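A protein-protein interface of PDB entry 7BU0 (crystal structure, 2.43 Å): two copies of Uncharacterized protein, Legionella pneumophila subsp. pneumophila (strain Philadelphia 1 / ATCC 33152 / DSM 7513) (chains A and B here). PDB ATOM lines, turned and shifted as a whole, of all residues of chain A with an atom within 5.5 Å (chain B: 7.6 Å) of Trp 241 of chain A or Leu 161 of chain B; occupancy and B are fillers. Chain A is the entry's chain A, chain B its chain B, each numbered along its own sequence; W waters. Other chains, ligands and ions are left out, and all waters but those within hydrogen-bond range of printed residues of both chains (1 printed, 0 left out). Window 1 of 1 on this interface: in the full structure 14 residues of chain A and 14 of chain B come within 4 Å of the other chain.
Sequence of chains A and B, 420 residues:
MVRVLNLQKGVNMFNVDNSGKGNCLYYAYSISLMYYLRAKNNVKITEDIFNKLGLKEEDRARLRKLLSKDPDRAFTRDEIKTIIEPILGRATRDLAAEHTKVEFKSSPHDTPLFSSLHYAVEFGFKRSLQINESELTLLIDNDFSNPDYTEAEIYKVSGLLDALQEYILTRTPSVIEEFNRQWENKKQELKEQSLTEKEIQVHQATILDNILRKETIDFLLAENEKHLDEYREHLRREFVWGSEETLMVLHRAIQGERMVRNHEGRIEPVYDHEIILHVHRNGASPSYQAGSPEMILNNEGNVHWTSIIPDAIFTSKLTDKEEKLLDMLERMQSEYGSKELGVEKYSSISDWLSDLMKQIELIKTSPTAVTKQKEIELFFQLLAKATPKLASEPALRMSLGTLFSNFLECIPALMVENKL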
ATOM      1  N   LYS A  21      23.991  14.411 -33.196  1.00  0.00           N
ATOM      2  CA  LYS A  21      22.639  14.952 -33.358  1.00  0.00           C
ATOM      3  C   LYS A  21      21.746  13.934 -34.050  1.00  0.00           C
ATOM      4  O   LYS A  21      20.980  14.250 -34.958  1.00  0.00           O
ATOM      5  CB  LYS A  21      22.682  16.257 -34.140  1.00  0.00           C
ATOM      6  CG  LYS A  21      23.297  17.413 -33.386  1.00  0.00           C
ATOM      7  CD  LYS A  21      24.762  17.566 -33.720  1.00  0.00           C
ATOM      8  CE  LYS A  21      25.157  19.028 -33.765  1.00  0.00           C
ATOM      9  NZ  LYS A  21      24.994  19.661 -32.426  1.00  0.00           N
ATOM     10  N   GLY A  22      21.847  12.682 -33.619  1.00  0.00           N
ATOM     11  CA  GLY A  22      21.150  11.583 -34.251  1.00  0.00           C
ATOM     12  C   GLY A  22      22.084  10.682 -35.016  1.00  0.00           C
ATOM     13  O   GLY A  22      21.651   9.640 -35.522  1.00  0.00           O
ATOM     14  N   ARG A  93      27.494   5.394 -42.222  1.00  0.00           N
ATOM     15  CA  ARG A  93      26.044   5.392 -42.392  1.00  0.00           C
ATOM     16  C   ARG A  93      25.662   4.891 -43.779  1.00  0.00           C
ATOM     17  O   ARG A  93      24.749   4.072 -43.927  1.00  0.00           O
ATOM     18  CB  ARG A  93      25.470   6.790 -42.142  1.00  0.00           C
ATOM     19  CG  ARG A  93      23.953   6.848 -42.285  1.00  0.00           C
ATOM     20  CD  ARG A  93      23.394   8.252 -42.090  1.00  0.00           C
ATOM     21  NE  ARG A  93      23.385   8.667 -40.690  1.00  0.00           N
ATOM     22  CZ  ARG A  93      22.448   8.329 -39.811  1.00  0.00           C
ATOM     23  NH1 ARG A  93      21.437   7.548 -40.176  1.00  0.00           N
ATOM     24  NH2 ARG A  93      22.529   8.763 -38.561  1.00  0.00           N
ATOM     25  N   GLU A 153      13.545  -1.778 -36.338  1.00  0.00           N
ATOM     26  CA  GLU A 153      13.582  -0.488 -37.022  1.00  0.00           C
ATOM     27  C   GLU A 153      12.600  -0.419 -38.188  1.00  0.00           C
ATOM     28  O   GLU A 153      12.098   0.668 -38.500  1.00  0.00           O
ATOM     29  CB  GLU A 153      15.004  -0.197 -37.504  1.00  0.00           C
ATOM     30  CG  GLU A 153      15.178   1.147 -38.197  1.00  0.00           C
ATOM     31  CD  GLU A 153      15.125   2.325 -37.236  1.00  0.00           C
ATOM     32  OE1 GLU A 153      15.200   2.107 -36.005  1.00  0.00           O
ATOM     33  OE2 GLU A 153      15.022   3.474 -37.721  1.00  0.00           O
ATOM     34  N   PHE A 239      20.727  12.025 -39.535  1.00  0.00           N
ATOM     35  CA  PHE A 239      20.248  12.144 -38.157  1.00  0.00           C
ATOM     36  C   PHE A 239      19.259  11.056 -37.751  1.00  0.00           C
ATOM     37  O   PHE A 239      18.763  11.105 -36.616  1.00  0.00           O
ATOM     38  CB  PHE A 239      19.596  13.504 -37.862  1.00  0.00           C
ATOM     39  CG  PHE A 239      20.407  14.680 -38.312  1.00  0.00           C
ATOM     40  CD1 PHE A 239      21.720  14.835 -37.900  1.00  0.00           C
ATOM     41  CD2 PHE A 239      19.854  15.637 -39.145  1.00  0.00           C
ATOM     42  CE1 PHE A 239      22.463  15.925 -38.305  1.00  0.00           C
ATOM     43  CE2 PHE A 239      20.592  16.727 -39.558  1.00  0.00           C
ATOM     44  CZ  PHE A 239      21.897  16.873 -39.135  1.00  0.00           C
ATOM     45  N   VAL A 240      18.942  10.092 -38.618  1.00  0.00           N
ATOM     46  CA  VAL A 240      18.068   8.997 -38.212  1.00  0.00           C
ATOM     47  C   VAL A 240      18.814   8.104 -37.229  1.00  0.00           C
ATOM     48  O   VAL A 240      19.951   7.686 -37.484  1.00  0.00           O
ATOM     49  CB  VAL A 240      17.580   8.214 -39.440  1.00  0.00           C
ATOM     50  CG1 VAL A 240      16.965   6.885 -39.027  1.00  0.00           C
ATOM     51  CG2 VAL A 240      16.573   9.043 -40.218  1.00  0.00           C
ATOM     52  N   TRP A 241      18.174   7.808 -36.099  1.00  0.00           N
ATOM     53  CA  TRP A 241      18.827   7.074 -35.022  1.00  0.00           C
ATOM     54  C   TRP A 241      19.153   5.649 -35.453  1.00  0.00           C
ATOM     55  O   TRP A 241      18.289   4.924 -35.956  1.00  0.00           O
ATOM     56  CB  TRP A 241      17.936   7.057 -33.776  1.00  0.00           C
ATOM     57  CG  TRP A 241      17.843   8.380 -33.057  1.00  0.00           C
ATOM     58  CD1 TRP A 241      18.150   9.613 -33.561  1.00  0.00           C
ATOM     59  CD2 TRP A 241      17.412   8.597 -31.705  1.00  0.00           C
ATOM     60  NE1 TRP A 241      17.937  10.580 -32.607  1.00  0.00           N
ATOM     61  CE2 TRP A 241      17.484   9.984 -31.460  1.00  0.00           C
ATOM     62  CE3 TRP A 241      16.973   7.753 -30.679  1.00  0.00           C
ATOM     63  CZ2 TRP A 241      17.142  10.546 -30.229  1.00  0.00           C
ATOM     64  CZ3 TRP A 241      16.628   8.312 -29.459  1.00  0.00           C
ATOM     65  CH2 TRP A 241      16.712   9.694 -29.245  1.00  0.00           C
ATOM     66  N   GLY A 242      20.408   5.249 -35.260  1.00  0.00           N
ATOM     67  CA  GLY A 242      20.802   3.891 -35.570  1.00  0.00           C
ATOM     68  C   GLY A 242      20.430   2.940 -34.444  1.00  0.00           C
ATOM     69  O   GLY A 242      20.593   3.242 -33.260  1.00  0.00           O
ATOM     70  N   SER A 243      19.921   1.776 -34.830  1.00  0.00           N
ATOM     71  CA  SER A 243      19.658   0.693 -33.899  1.00  0.00           C
ATOM     72  C   SER A 243      20.740  -0.370 -34.043  1.00  0.00           C
ATOM     73  O   SER A 243      21.508  -0.384 -35.007  1.00  0.00           O
ATOM     74  CB  SER A 243      18.266   0.100 -34.133  1.00  0.00           C
ATOM     75  OG  SER A 243      18.236  -0.717 -35.291  1.00  0.00           O
ATOM     76  N   ASN A 302      18.934   4.046 -24.382  1.00  0.00           N
ATOM     77  CA  ASN A 302      18.190   3.988 -25.644  1.00  0.00           C
ATOM     78  C   ASN A 302      18.030   5.368 -26.285  1.00  0.00           C
ATOM     79  O   ASN A 302      17.070   5.614 -27.022  1.00  0.00           O
ATOM     80  CB  ASN A 302      16.823   3.318 -25.460  1.00  0.00           C
ATOM     81  CG  ASN A 302      16.797   1.898 -25.985  1.00  0.00           C
ATOM     82  OD1 ASN A 302      17.690   1.481 -26.720  1.00  0.00           O
ATOM     83  ND2 ASN A 302      15.774   1.144 -25.605  1.00  0.00           N
ATOM     84  N   VAL A 303      18.951   6.288 -26.001  1.00  0.00           N
ATOM     85  CA  VAL A 303      18.929   7.607 -26.631  1.00  0.00           C
ATOM     86  C   VAL A 303      20.286   8.050 -27.151  1.00  0.00           C
ATOM     87  O   VAL A 303      20.345   9.002 -27.952  1.00  0.00           O
ATOM     88  CB  VAL A 303      18.367   8.673 -25.661  1.00  0.00           C
ATOM     89  CG1 VAL A 303      16.980   8.294 -25.166  1.00  0.00           C
ATOM     90  CG2 VAL A 303      19.325   8.891 -24.500  1.00  0.00           C
ATOM     91  N   LEU B 117       6.637  14.021 -21.286  1.00  0.00           N
ATOM     92  CA  LEU B 117       7.924  14.524 -21.753  1.00  0.00           C
ATOM     93  C   LEU B 117       8.891  14.782 -20.604  1.00  0.00           C
ATOM     94  O   LEU B 117      10.106  14.656 -20.789  1.00  0.00           O
ATOM     95  CB  LEU B 117       7.724  15.796 -22.578  1.00  0.00           C
ATOM     96  CG  LEU B 117       8.985  16.443 -23.161  1.00  0.00           C
ATOM     97  CD1 LEU B 117       9.789  15.451 -23.996  1.00  0.00           C
ATOM     98  CD2 LEU B 117       8.637  17.691 -23.969  1.00  0.00           C
ATOM     99  N   ALA B 120      11.886  12.351 -20.065  1.00  0.00           N
ATOM    100  CA  ALA B 120      13.113  12.566 -20.828  1.00  0.00           C
ATOM    101  C   ALA B 120      13.889  13.772 -20.314  1.00  0.00           C
ATOM    102  O   ALA B 120      15.126  13.761 -20.296  1.00  0.00           O
ATOM    103  CB  ALA B 120      12.791  12.746 -22.309  1.00  0.00           C
ATOM    104  N   VAL B 121      13.182  14.827 -19.906  1.00  0.00           N
ATOM    105  CA  VAL B 121      13.862  16.025 -19.421  1.00  0.00           C
ATOM    106  C   VAL B 121      14.637  15.723 -18.144  1.00  0.00           C
ATOM    107  O   VAL B 121      15.790  16.144 -17.989  1.00  0.00           O
ATOM    108  CB  VAL B 121      12.851  17.168 -19.219  1.00  0.00           C
ATOM    109  CG1 VAL B 121      13.545  18.373 -18.618  1.00  0.00           C
ATOM    110  CG2 VAL B 121      12.199  17.534 -20.544  1.00  0.00           C
ATOM    111  N   PHE B 144      15.472   6.111 -17.908  1.00  0.00           N
ATOM    112  CA  PHE B 144      14.694   6.174 -19.151  1.00  0.00           C
ATOM    113  C   PHE B 144      14.291   4.786 -19.643  1.00  0.00           C
ATOM    114  O   PHE B 144      14.336   4.489 -20.840  1.00  0.00           O
ATOM    115  CB  PHE B 144      15.454   6.936 -20.242  1.00  0.00           C
ATOM    116  CG  PHE B 144      14.556   7.563 -21.277  1.00  0.00           C
ATOM    117  CD1 PHE B 144      13.681   8.577 -20.927  1.00  0.00           C
ATOM    118  CD2 PHE B 144      14.589   7.139 -22.597  1.00  0.00           C
ATOM    119  CE1 PHE B 144      12.854   9.158 -21.871  1.00  0.00           C
ATOM    120  CE2 PHE B 144      13.761   7.718 -23.546  1.00  0.00           C
ATOM    121  CZ  PHE B 144      12.893   8.729 -23.181  1.00  0.00           C
ATOM    122  N   THR B 150       8.024   6.039 -21.941  1.00  0.00           N
ATOM    123  CA  THR B 150       8.756   6.048 -23.207  1.00  0.00           C
ATOM    124  C   THR B 150       7.863   5.765 -24.407  1.00  0.00           C
ATOM    125  O   THR B 150       8.263   6.057 -25.537  1.00  0.00           O
ATOM    126  CB  THR B 150       9.904   5.034 -23.183  1.00  0.00           C
ATOM    127  OG1 THR B 150       9.385   3.710 -23.004  1.00  0.00           O
ATOM    128  CG2 THR B 150      10.883   5.356 -22.067  1.00  0.00           C
ATOM    129  N   ILE B 154       4.895  11.928 -27.829  1.00  0.00           N
ATOM    130  CA  ILE B 154       5.880  13.000 -27.947  1.00  0.00           C
ATOM    131  C   ILE B 154       7.235  12.465 -28.400  1.00  0.00           C
ATOM    132  O   ILE B 154       7.955  13.138 -29.149  1.00  0.00           O
ATOM    133  CB  ILE B 154       5.978  13.769 -26.612  1.00  0.00           C
ATOM    134  CG1 ILE B 154       6.941  14.946 -26.739  1.00  0.00           C
ATOM    135  CG2 ILE B 154       6.385  12.846 -25.470  1.00  0.00           C
ATOM    136  CD1 ILE B 154       6.544  15.927 -27.815  1.00  0.00           C
ATOM    137  N   TYR B 155       7.595  11.247 -27.989  1.00  0.00           N
ATOM    138  CA  TYR B 155       8.880  10.664 -28.354  1.00  0.00           C
ATOM    139  C   TYR B 155       8.893  10.094 -29.766  1.00  0.00           C
ATOM    140  O   TYR B 155       9.954   9.668 -30.233  1.00  0.00           O
ATOM    141  CB  TYR B 155       9.275   9.584 -27.344  1.00  0.00           C
ATOM    142  CG  TYR B 155       9.389  10.134 -25.946  1.00  0.00           C
ATOM    143  CD1 TYR B 155      10.306  11.130 -25.654  1.00  0.00           C
ATOM    144  CD2 TYR B 155       8.571   9.675 -24.924  1.00  0.00           C
ATOM    145  CE1 TYR B 155      10.408  11.651 -24.388  1.00  0.00           C
ATOM    146  CE2 TYR B 155       8.670  10.190 -23.648  1.00  0.00           C
ATOM    147  CZ  TYR B 155       9.593  11.175 -23.383  1.00  0.00           C
ATOM    148  OH  TYR B 155       9.696  11.692 -22.109  1.00  0.00           O
ATOM    149  N   LYS B 156       7.752  10.068 -30.449  1.00  0.00           N
ATOM    150  CA  LYS B 156       7.702   9.676 -31.849  1.00  0.00           C
ATOM    151  C   LYS B 156       7.747  10.869 -32.796  1.00  0.00           C
ATOM    152  O   LYS B 156       7.689  10.674 -34.015  1.00  0.00           O
ATOM    153  CB  LYS B 156       6.450   8.837 -32.120  1.00  0.00           C
ATOM    154  CG  LYS B 156       6.440   7.507 -31.382  1.00  0.00           C
ATOM    155  CD  LYS B 156       5.247   6.658 -31.785  1.00  0.00           C
ATOM    156  CE  LYS B 156       5.243   5.335 -31.039  1.00  0.00           C
ATOM    157  NZ  LYS B 156       4.802   5.499 -29.623  1.00  0.00           N
ATOM    158  N   VAL B 157       7.848  12.089 -32.273  1.00  0.00           N
ATOM    159  CA  VAL B 157       7.993  13.268 -33.118  1.00  0.00           C
ATOM    160  C   VAL B 157       9.448  13.366 -33.560  1.00  0.00           C
ATOM    161  O   VAL B 157      10.364  13.355 -32.729  1.00  0.00           O
ATOM    162  CB  VAL B 157       7.538  14.536 -32.377  1.00  0.00           C
ATOM    163  CG1 VAL B 157       7.740  15.767 -33.250  1.00  0.00           C
ATOM    164  CG2 VAL B 157       6.072  14.416 -31.965  1.00  0.00           C
ATOM    165  N   SER B 158       9.659  13.478 -34.872  1.00  0.00           N
ATOM    166  CA  SER B 158      11.003  13.395 -35.432  1.00  0.00           C
ATOM    167  C   SER B 158      11.868  14.558 -34.964  1.00  0.00           C
ATOM    168  O   SER B 158      11.492  15.727 -35.095  1.00  0.00           O
ATOM    169  CB  SER B 158      10.936  13.371 -36.960  1.00  0.00           C
ATOM    170  OG  SER B 158      11.169  14.661 -37.501  1.00  0.00           O
ATOM    171  N   GLY B 159      13.043  14.228 -34.433  1.00  0.00           N
ATOM    172  CA  GLY B 159      14.003  15.222 -34.022  1.00  0.00           C
ATOM    173  C   GLY B 159      13.709  15.923 -32.715  1.00  0.00           C
ATOM    174  O   GLY B 159      14.542  16.719 -32.266  1.00  0.00           O
ATOM    175  N   LEU B 160      12.552  15.678 -32.093  1.00  0.00           N
ATOM    176  CA  LEU B 160      12.237  16.396 -30.863  1.00  0.00           C
ATOM    177  C   LEU B 160      13.270  16.107 -29.785  1.00  0.00           C
ATOM    178  O   LEU B 160      13.722  17.021 -29.085  1.00  0.00           O
ATOM    179  CB  LEU B 160      10.841  16.041 -30.357  1.00  0.00           C
ATOM    180  CG  LEU B 160      10.576  16.831 -29.070  1.00  0.00           C
ATOM    181  CD1 LEU B 160       9.639  18.009 -29.315  1.00  0.00           C
ATOM    182  CD2 LEU B 160      10.091  15.943 -27.942  1.00  0.00           C
ATOM    183  N   LEU B 161      13.648  14.835 -29.629  1.00  0.00           N
ATOM    184  CA  LEU B 161      14.652  14.486 -28.631  1.00  0.00           C
ATOM    185  C   LEU B 161      16.025  15.035 -28.998  1.00  0.00           C
ATOM    186  O   LEU B 161      16.818  15.354 -28.105  1.00  0.00           O
ATOM    187  CB  LEU B 161      14.710  12.972 -28.454  1.00  0.00           C
ATOM    188  CG  LEU B 161      13.637  12.417 -27.517  1.00  0.00           C
ATOM    189  CD1 LEU B 161      13.607  10.898 -27.564  1.00  0.00           C
ATOM    190  CD2 LEU B 161      13.863  12.906 -26.096  1.00  0.00           C
ATOM    191  N   ASP B 162      16.327  15.153 -30.295  1.00  0.00           N
ATOM    192  CA  ASP B 162      17.545  15.847 -30.700  1.00  0.00           C
ATOM    193  C   ASP B 162      17.529  17.288 -30.211  1.00  0.00           C
ATOM    194  O   ASP B 162      18.497  17.764 -29.604  1.00  0.00           O
ATOM    195  CB  ASP B 162      17.708  15.805 -32.222  1.00  0.00           C
ATOM    196  CG  ASP B 162      17.849  14.397 -32.758  1.00  0.00           C
ATOM    197  OD1 ASP B 162      18.453  13.553 -32.062  1.00  0.00           O
ATOM    198  OD2 ASP B 162      17.363  14.138 -33.880  1.00  0.00           O
ATOM    199  N   ALA B 163      16.429  18.001 -30.473  1.00  0.00           N
ATOM    200  CA  ALA B 163      16.313  19.383 -30.021  1.00  0.00           C
ATOM    201  C   ALA B 163      16.312  19.473 -28.501  1.00  0.00           C
ATOM    202  O   ALA B 163      16.897  20.401 -27.926  1.00  0.00           O
ATOM    203  CB  ALA B 163      15.050  20.020 -30.598  1.00  0.00           C
ATOM    204  N   LEU B 164      15.658  18.522 -27.829  1.00  0.00           N
ATOM    205  CA  LEU B 164      15.670  18.529 -26.371  1.00  0.00           C
ATOM    206  C   LEU B 164      17.076  18.324 -25.831  1.00  0.00           C
ATOM    207  O   LEU B 164      17.428  18.876 -24.781  1.00  0.00           O
ATOM    208  CB  LEU B 164      14.737  17.450 -25.820  1.00  0.00           C
ATOM    209  CG  LEU B 164      14.792  17.295 -24.296  1.00  0.00           C
ATOM    210  CD1 LEU B 164      14.354  18.574 -23.604  1.00  0.00           C
ATOM    211  CD2 LEU B 164      13.962  16.110 -23.816  1.00  0.00           C
ATOM    212  N   GLN B 165      17.905  17.564 -26.547  1.00  0.00           N
ATOM    213  CA  GLN B 165      19.250  17.300 -26.057  1.00  0.00           C
ATOM    214  C   GLN B 165      20.123  18.545 -26.137  1.00  0.00           C
ATOM    215  O   GLN B 165      20.934  18.801 -25.240  1.00  0.00           O
ATOM    216  CB  GLN B 165      19.873  16.155 -26.855  1.00  0.00           C
ATOM    217  CG  GLN B 165      21.340  15.908 -26.554  1.00  0.00           C
ATOM    218  CD  GLN B 165      21.638  15.855 -25.067  1.00  0.00           C
ATOM    219  OE1 GLN B 165      20.910  15.231 -24.293  1.00  0.00           O
ATOM    220  NE2 GLN B 165      22.715  16.514 -24.662  1.00  0.00           N
ATOM    221  N   GLU B 166      19.948  19.351 -27.185  1.00  0.00           N
ATOM    222  CA  GLU B 166      20.742  20.565 -27.311  1.00  0.00           C
ATOM    223  C   GLU B 166      20.249  21.668 -26.386  1.00  0.00           C
ATOM    224  O   GLU B 166      21.048  22.500 -25.940  1.00  0.00           O
ATOM    225  CB  GLU B 166      20.713  21.059 -28.756  1.00  0.00           C
ATOM    226  CG  GLU B 166      21.556  20.241 -29.708  1.00  0.00           C
ATOM    227  CD  GLU B 166      23.040  20.337 -29.407  1.00  0.00           C
ATOM    228  OE1 GLU B 166      23.447  21.234 -28.638  1.00  0.00           O
ATOM    229  OE2 GLU B 166      23.804  19.510 -29.947  1.00  0.00           O
ATOM    230  N   TYR B 167      18.952  21.694 -26.090  1.00  0.00           N
ATOM    231  CA  TYR B 167      18.429  22.629 -25.102  1.00  0.00           C
ATOM    232  C   TYR B 167      18.976  22.318 -23.713  1.00  0.00           C
ATOM    233  O   TYR B 167      19.423  23.217 -22.992  1.00  0.00           O
ATOM    234  CB  TYR B 167      16.899  22.582 -25.122  1.00  0.00           C
ATOM    235  CG  TYR B 167      16.201  23.340 -24.016  1.00  0.00           C
ATOM    236  CD1 TYR B 167      15.923  22.730 -22.798  1.00  0.00           C
ATOM    237  CD2 TYR B 167      15.780  24.651 -24.203  1.00  0.00           C
ATOM    238  CE1 TYR B 167      15.270  23.409 -21.790  1.00  0.00           C
ATOM    239  CE2 TYR B 167      15.123  25.337 -23.201  1.00  0.00           C
ATOM    240  CZ  TYR B 167      14.868  24.710 -22.000  1.00  0.00           C
ATOM    241  OH  TYR B 167      14.223  25.401 -21.004  1.00  0.00           O
ATOM    242  N   ILE B 168      18.958  21.039 -23.330  1.00  0.00           N
ATOM    243  CA  ILE B 168      19.365  20.645 -21.985  1.00  0.00           C
ATOM    244  C   ILE B 168      20.845  20.917 -21.768  1.00  0.00           C
ATOM    245  O   ILE B 168      21.248  21.438 -20.719  1.00  0.00           O
ATOM    246  CB  ILE B 168      19.035  19.159 -21.748  1.00  0.00           C
ATOM    247  CG1 ILE B 168      17.543  18.968 -21.477  1.00  0.00           C
ATOM    248  CG2 ILE B 168      19.874  18.593 -20.608  1.00  0.00           C
ATOM    249  CD1 ILE B 168      17.151  17.521 -21.282  1.00  0.00           C
ATOM    250  N   PHE B 219      10.916  24.712 -22.442  1.00  0.00           N
ATOM    251  CA  PHE B 219      11.338  24.115 -23.703  1.00  0.00           C
ATOM    252  C   PHE B 219      10.205  24.125 -24.724  1.00  0.00           C
ATOM    253  O   PHE B 219      10.398  24.514 -25.881  1.00  0.00           O
ATOM    254  CB  PHE B 219      11.838  22.692 -23.441  1.00  0.00           C
ATOM    255  CG  PHE B 219      12.074  21.877 -24.681  1.00  0.00           C
ATOM    256  CD1 PHE B 219      13.176  22.111 -25.487  1.00  0.00           C
ATOM    257  CD2 PHE B 219      11.213  20.847 -25.019  1.00  0.00           C
ATOM    258  CE1 PHE B 219      13.401  21.347 -26.617  1.00  0.00           C
ATOM    259  CE2 PHE B 219      11.432  20.081 -26.147  1.00  0.00           C
ATOM    260  CZ  PHE B 219      12.527  20.331 -26.948  1.00  0.00           C
HETATM  261  O   HOH W   1      16.347  12.318 -35.709  1.00  0.00           O
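The indole nitrogen (NE1) of Trp 241 of chain A lies within hydrogen-bond range of the side-chain carboxylate (OD1) of Asp 162 of chain B, 3.1 Å away.
The side-chain carboxylate (OE2) of Glu 166 of chain B lies within salt-bridge range of the side-chain amino group (NZ) of Lys 21 of chain A (2.8 Å).
Water W1 bridges the side-chain carboxylate of Asp 162 of chain B and the backbone carbonyl oxygen of Phe 239 of chain A.
Trp 241 of chain A touches just these residues of chain B: Leu 161 (3.7 Å) and Asp 162 (3.1 Å).
Leu 161 of chain B touches just one residue of chain A: Trp 241.
Of the printed residues of chain B, Lys 21 of chain A touches Asp 162 and Glu 166.
Printed residues of chain A within 4 Å of Asp 162 of chain B: Lys 21, Gly 22 and Trp 241.
Of the printed residues of chain B, Val 303 of chain A touches Phe 144 (3.6 Å).
Printed residues of chain B within 4 Å of Gly 22 of chain A: Asp 162.
The nearest residue of chain B that does not touch Trp 241 of chain A is Gly 159 of chain B (6.2 Å).
The nearest printed residue of chain A that does not touch Asp 162 of chain B is Phe 239 of chain A (4.3 Å).
The backbone carbonyl oxygen of Gly 22 of chain A is in hydrogen-bond range of the guanidinium group of Arg 93 of chain A (3.3 Å).
Of the 21 printed residues of chain B, 4 touch a printed residue of chain A.
Among the printed residues, 6 pairs touch across the chains.
Among the printed residues, Asp or Glu carboxylates within 4 Å of a Lys or Arg side-chain nitrogen of the other chain: Lys 21 of chain A with Glu 166 of chain B (2.8 Å).
Among the printed residues, merely in contact across the chains: Val 303 of chain A with Phe 144 of chain B, Trp 241 of chain A with Leu 161 of chain B, Lys 21 of chain A with Asp 162 of chain B and Gly 22 of chain A with Asp 162 of chain B.
No position is printed for both chains.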
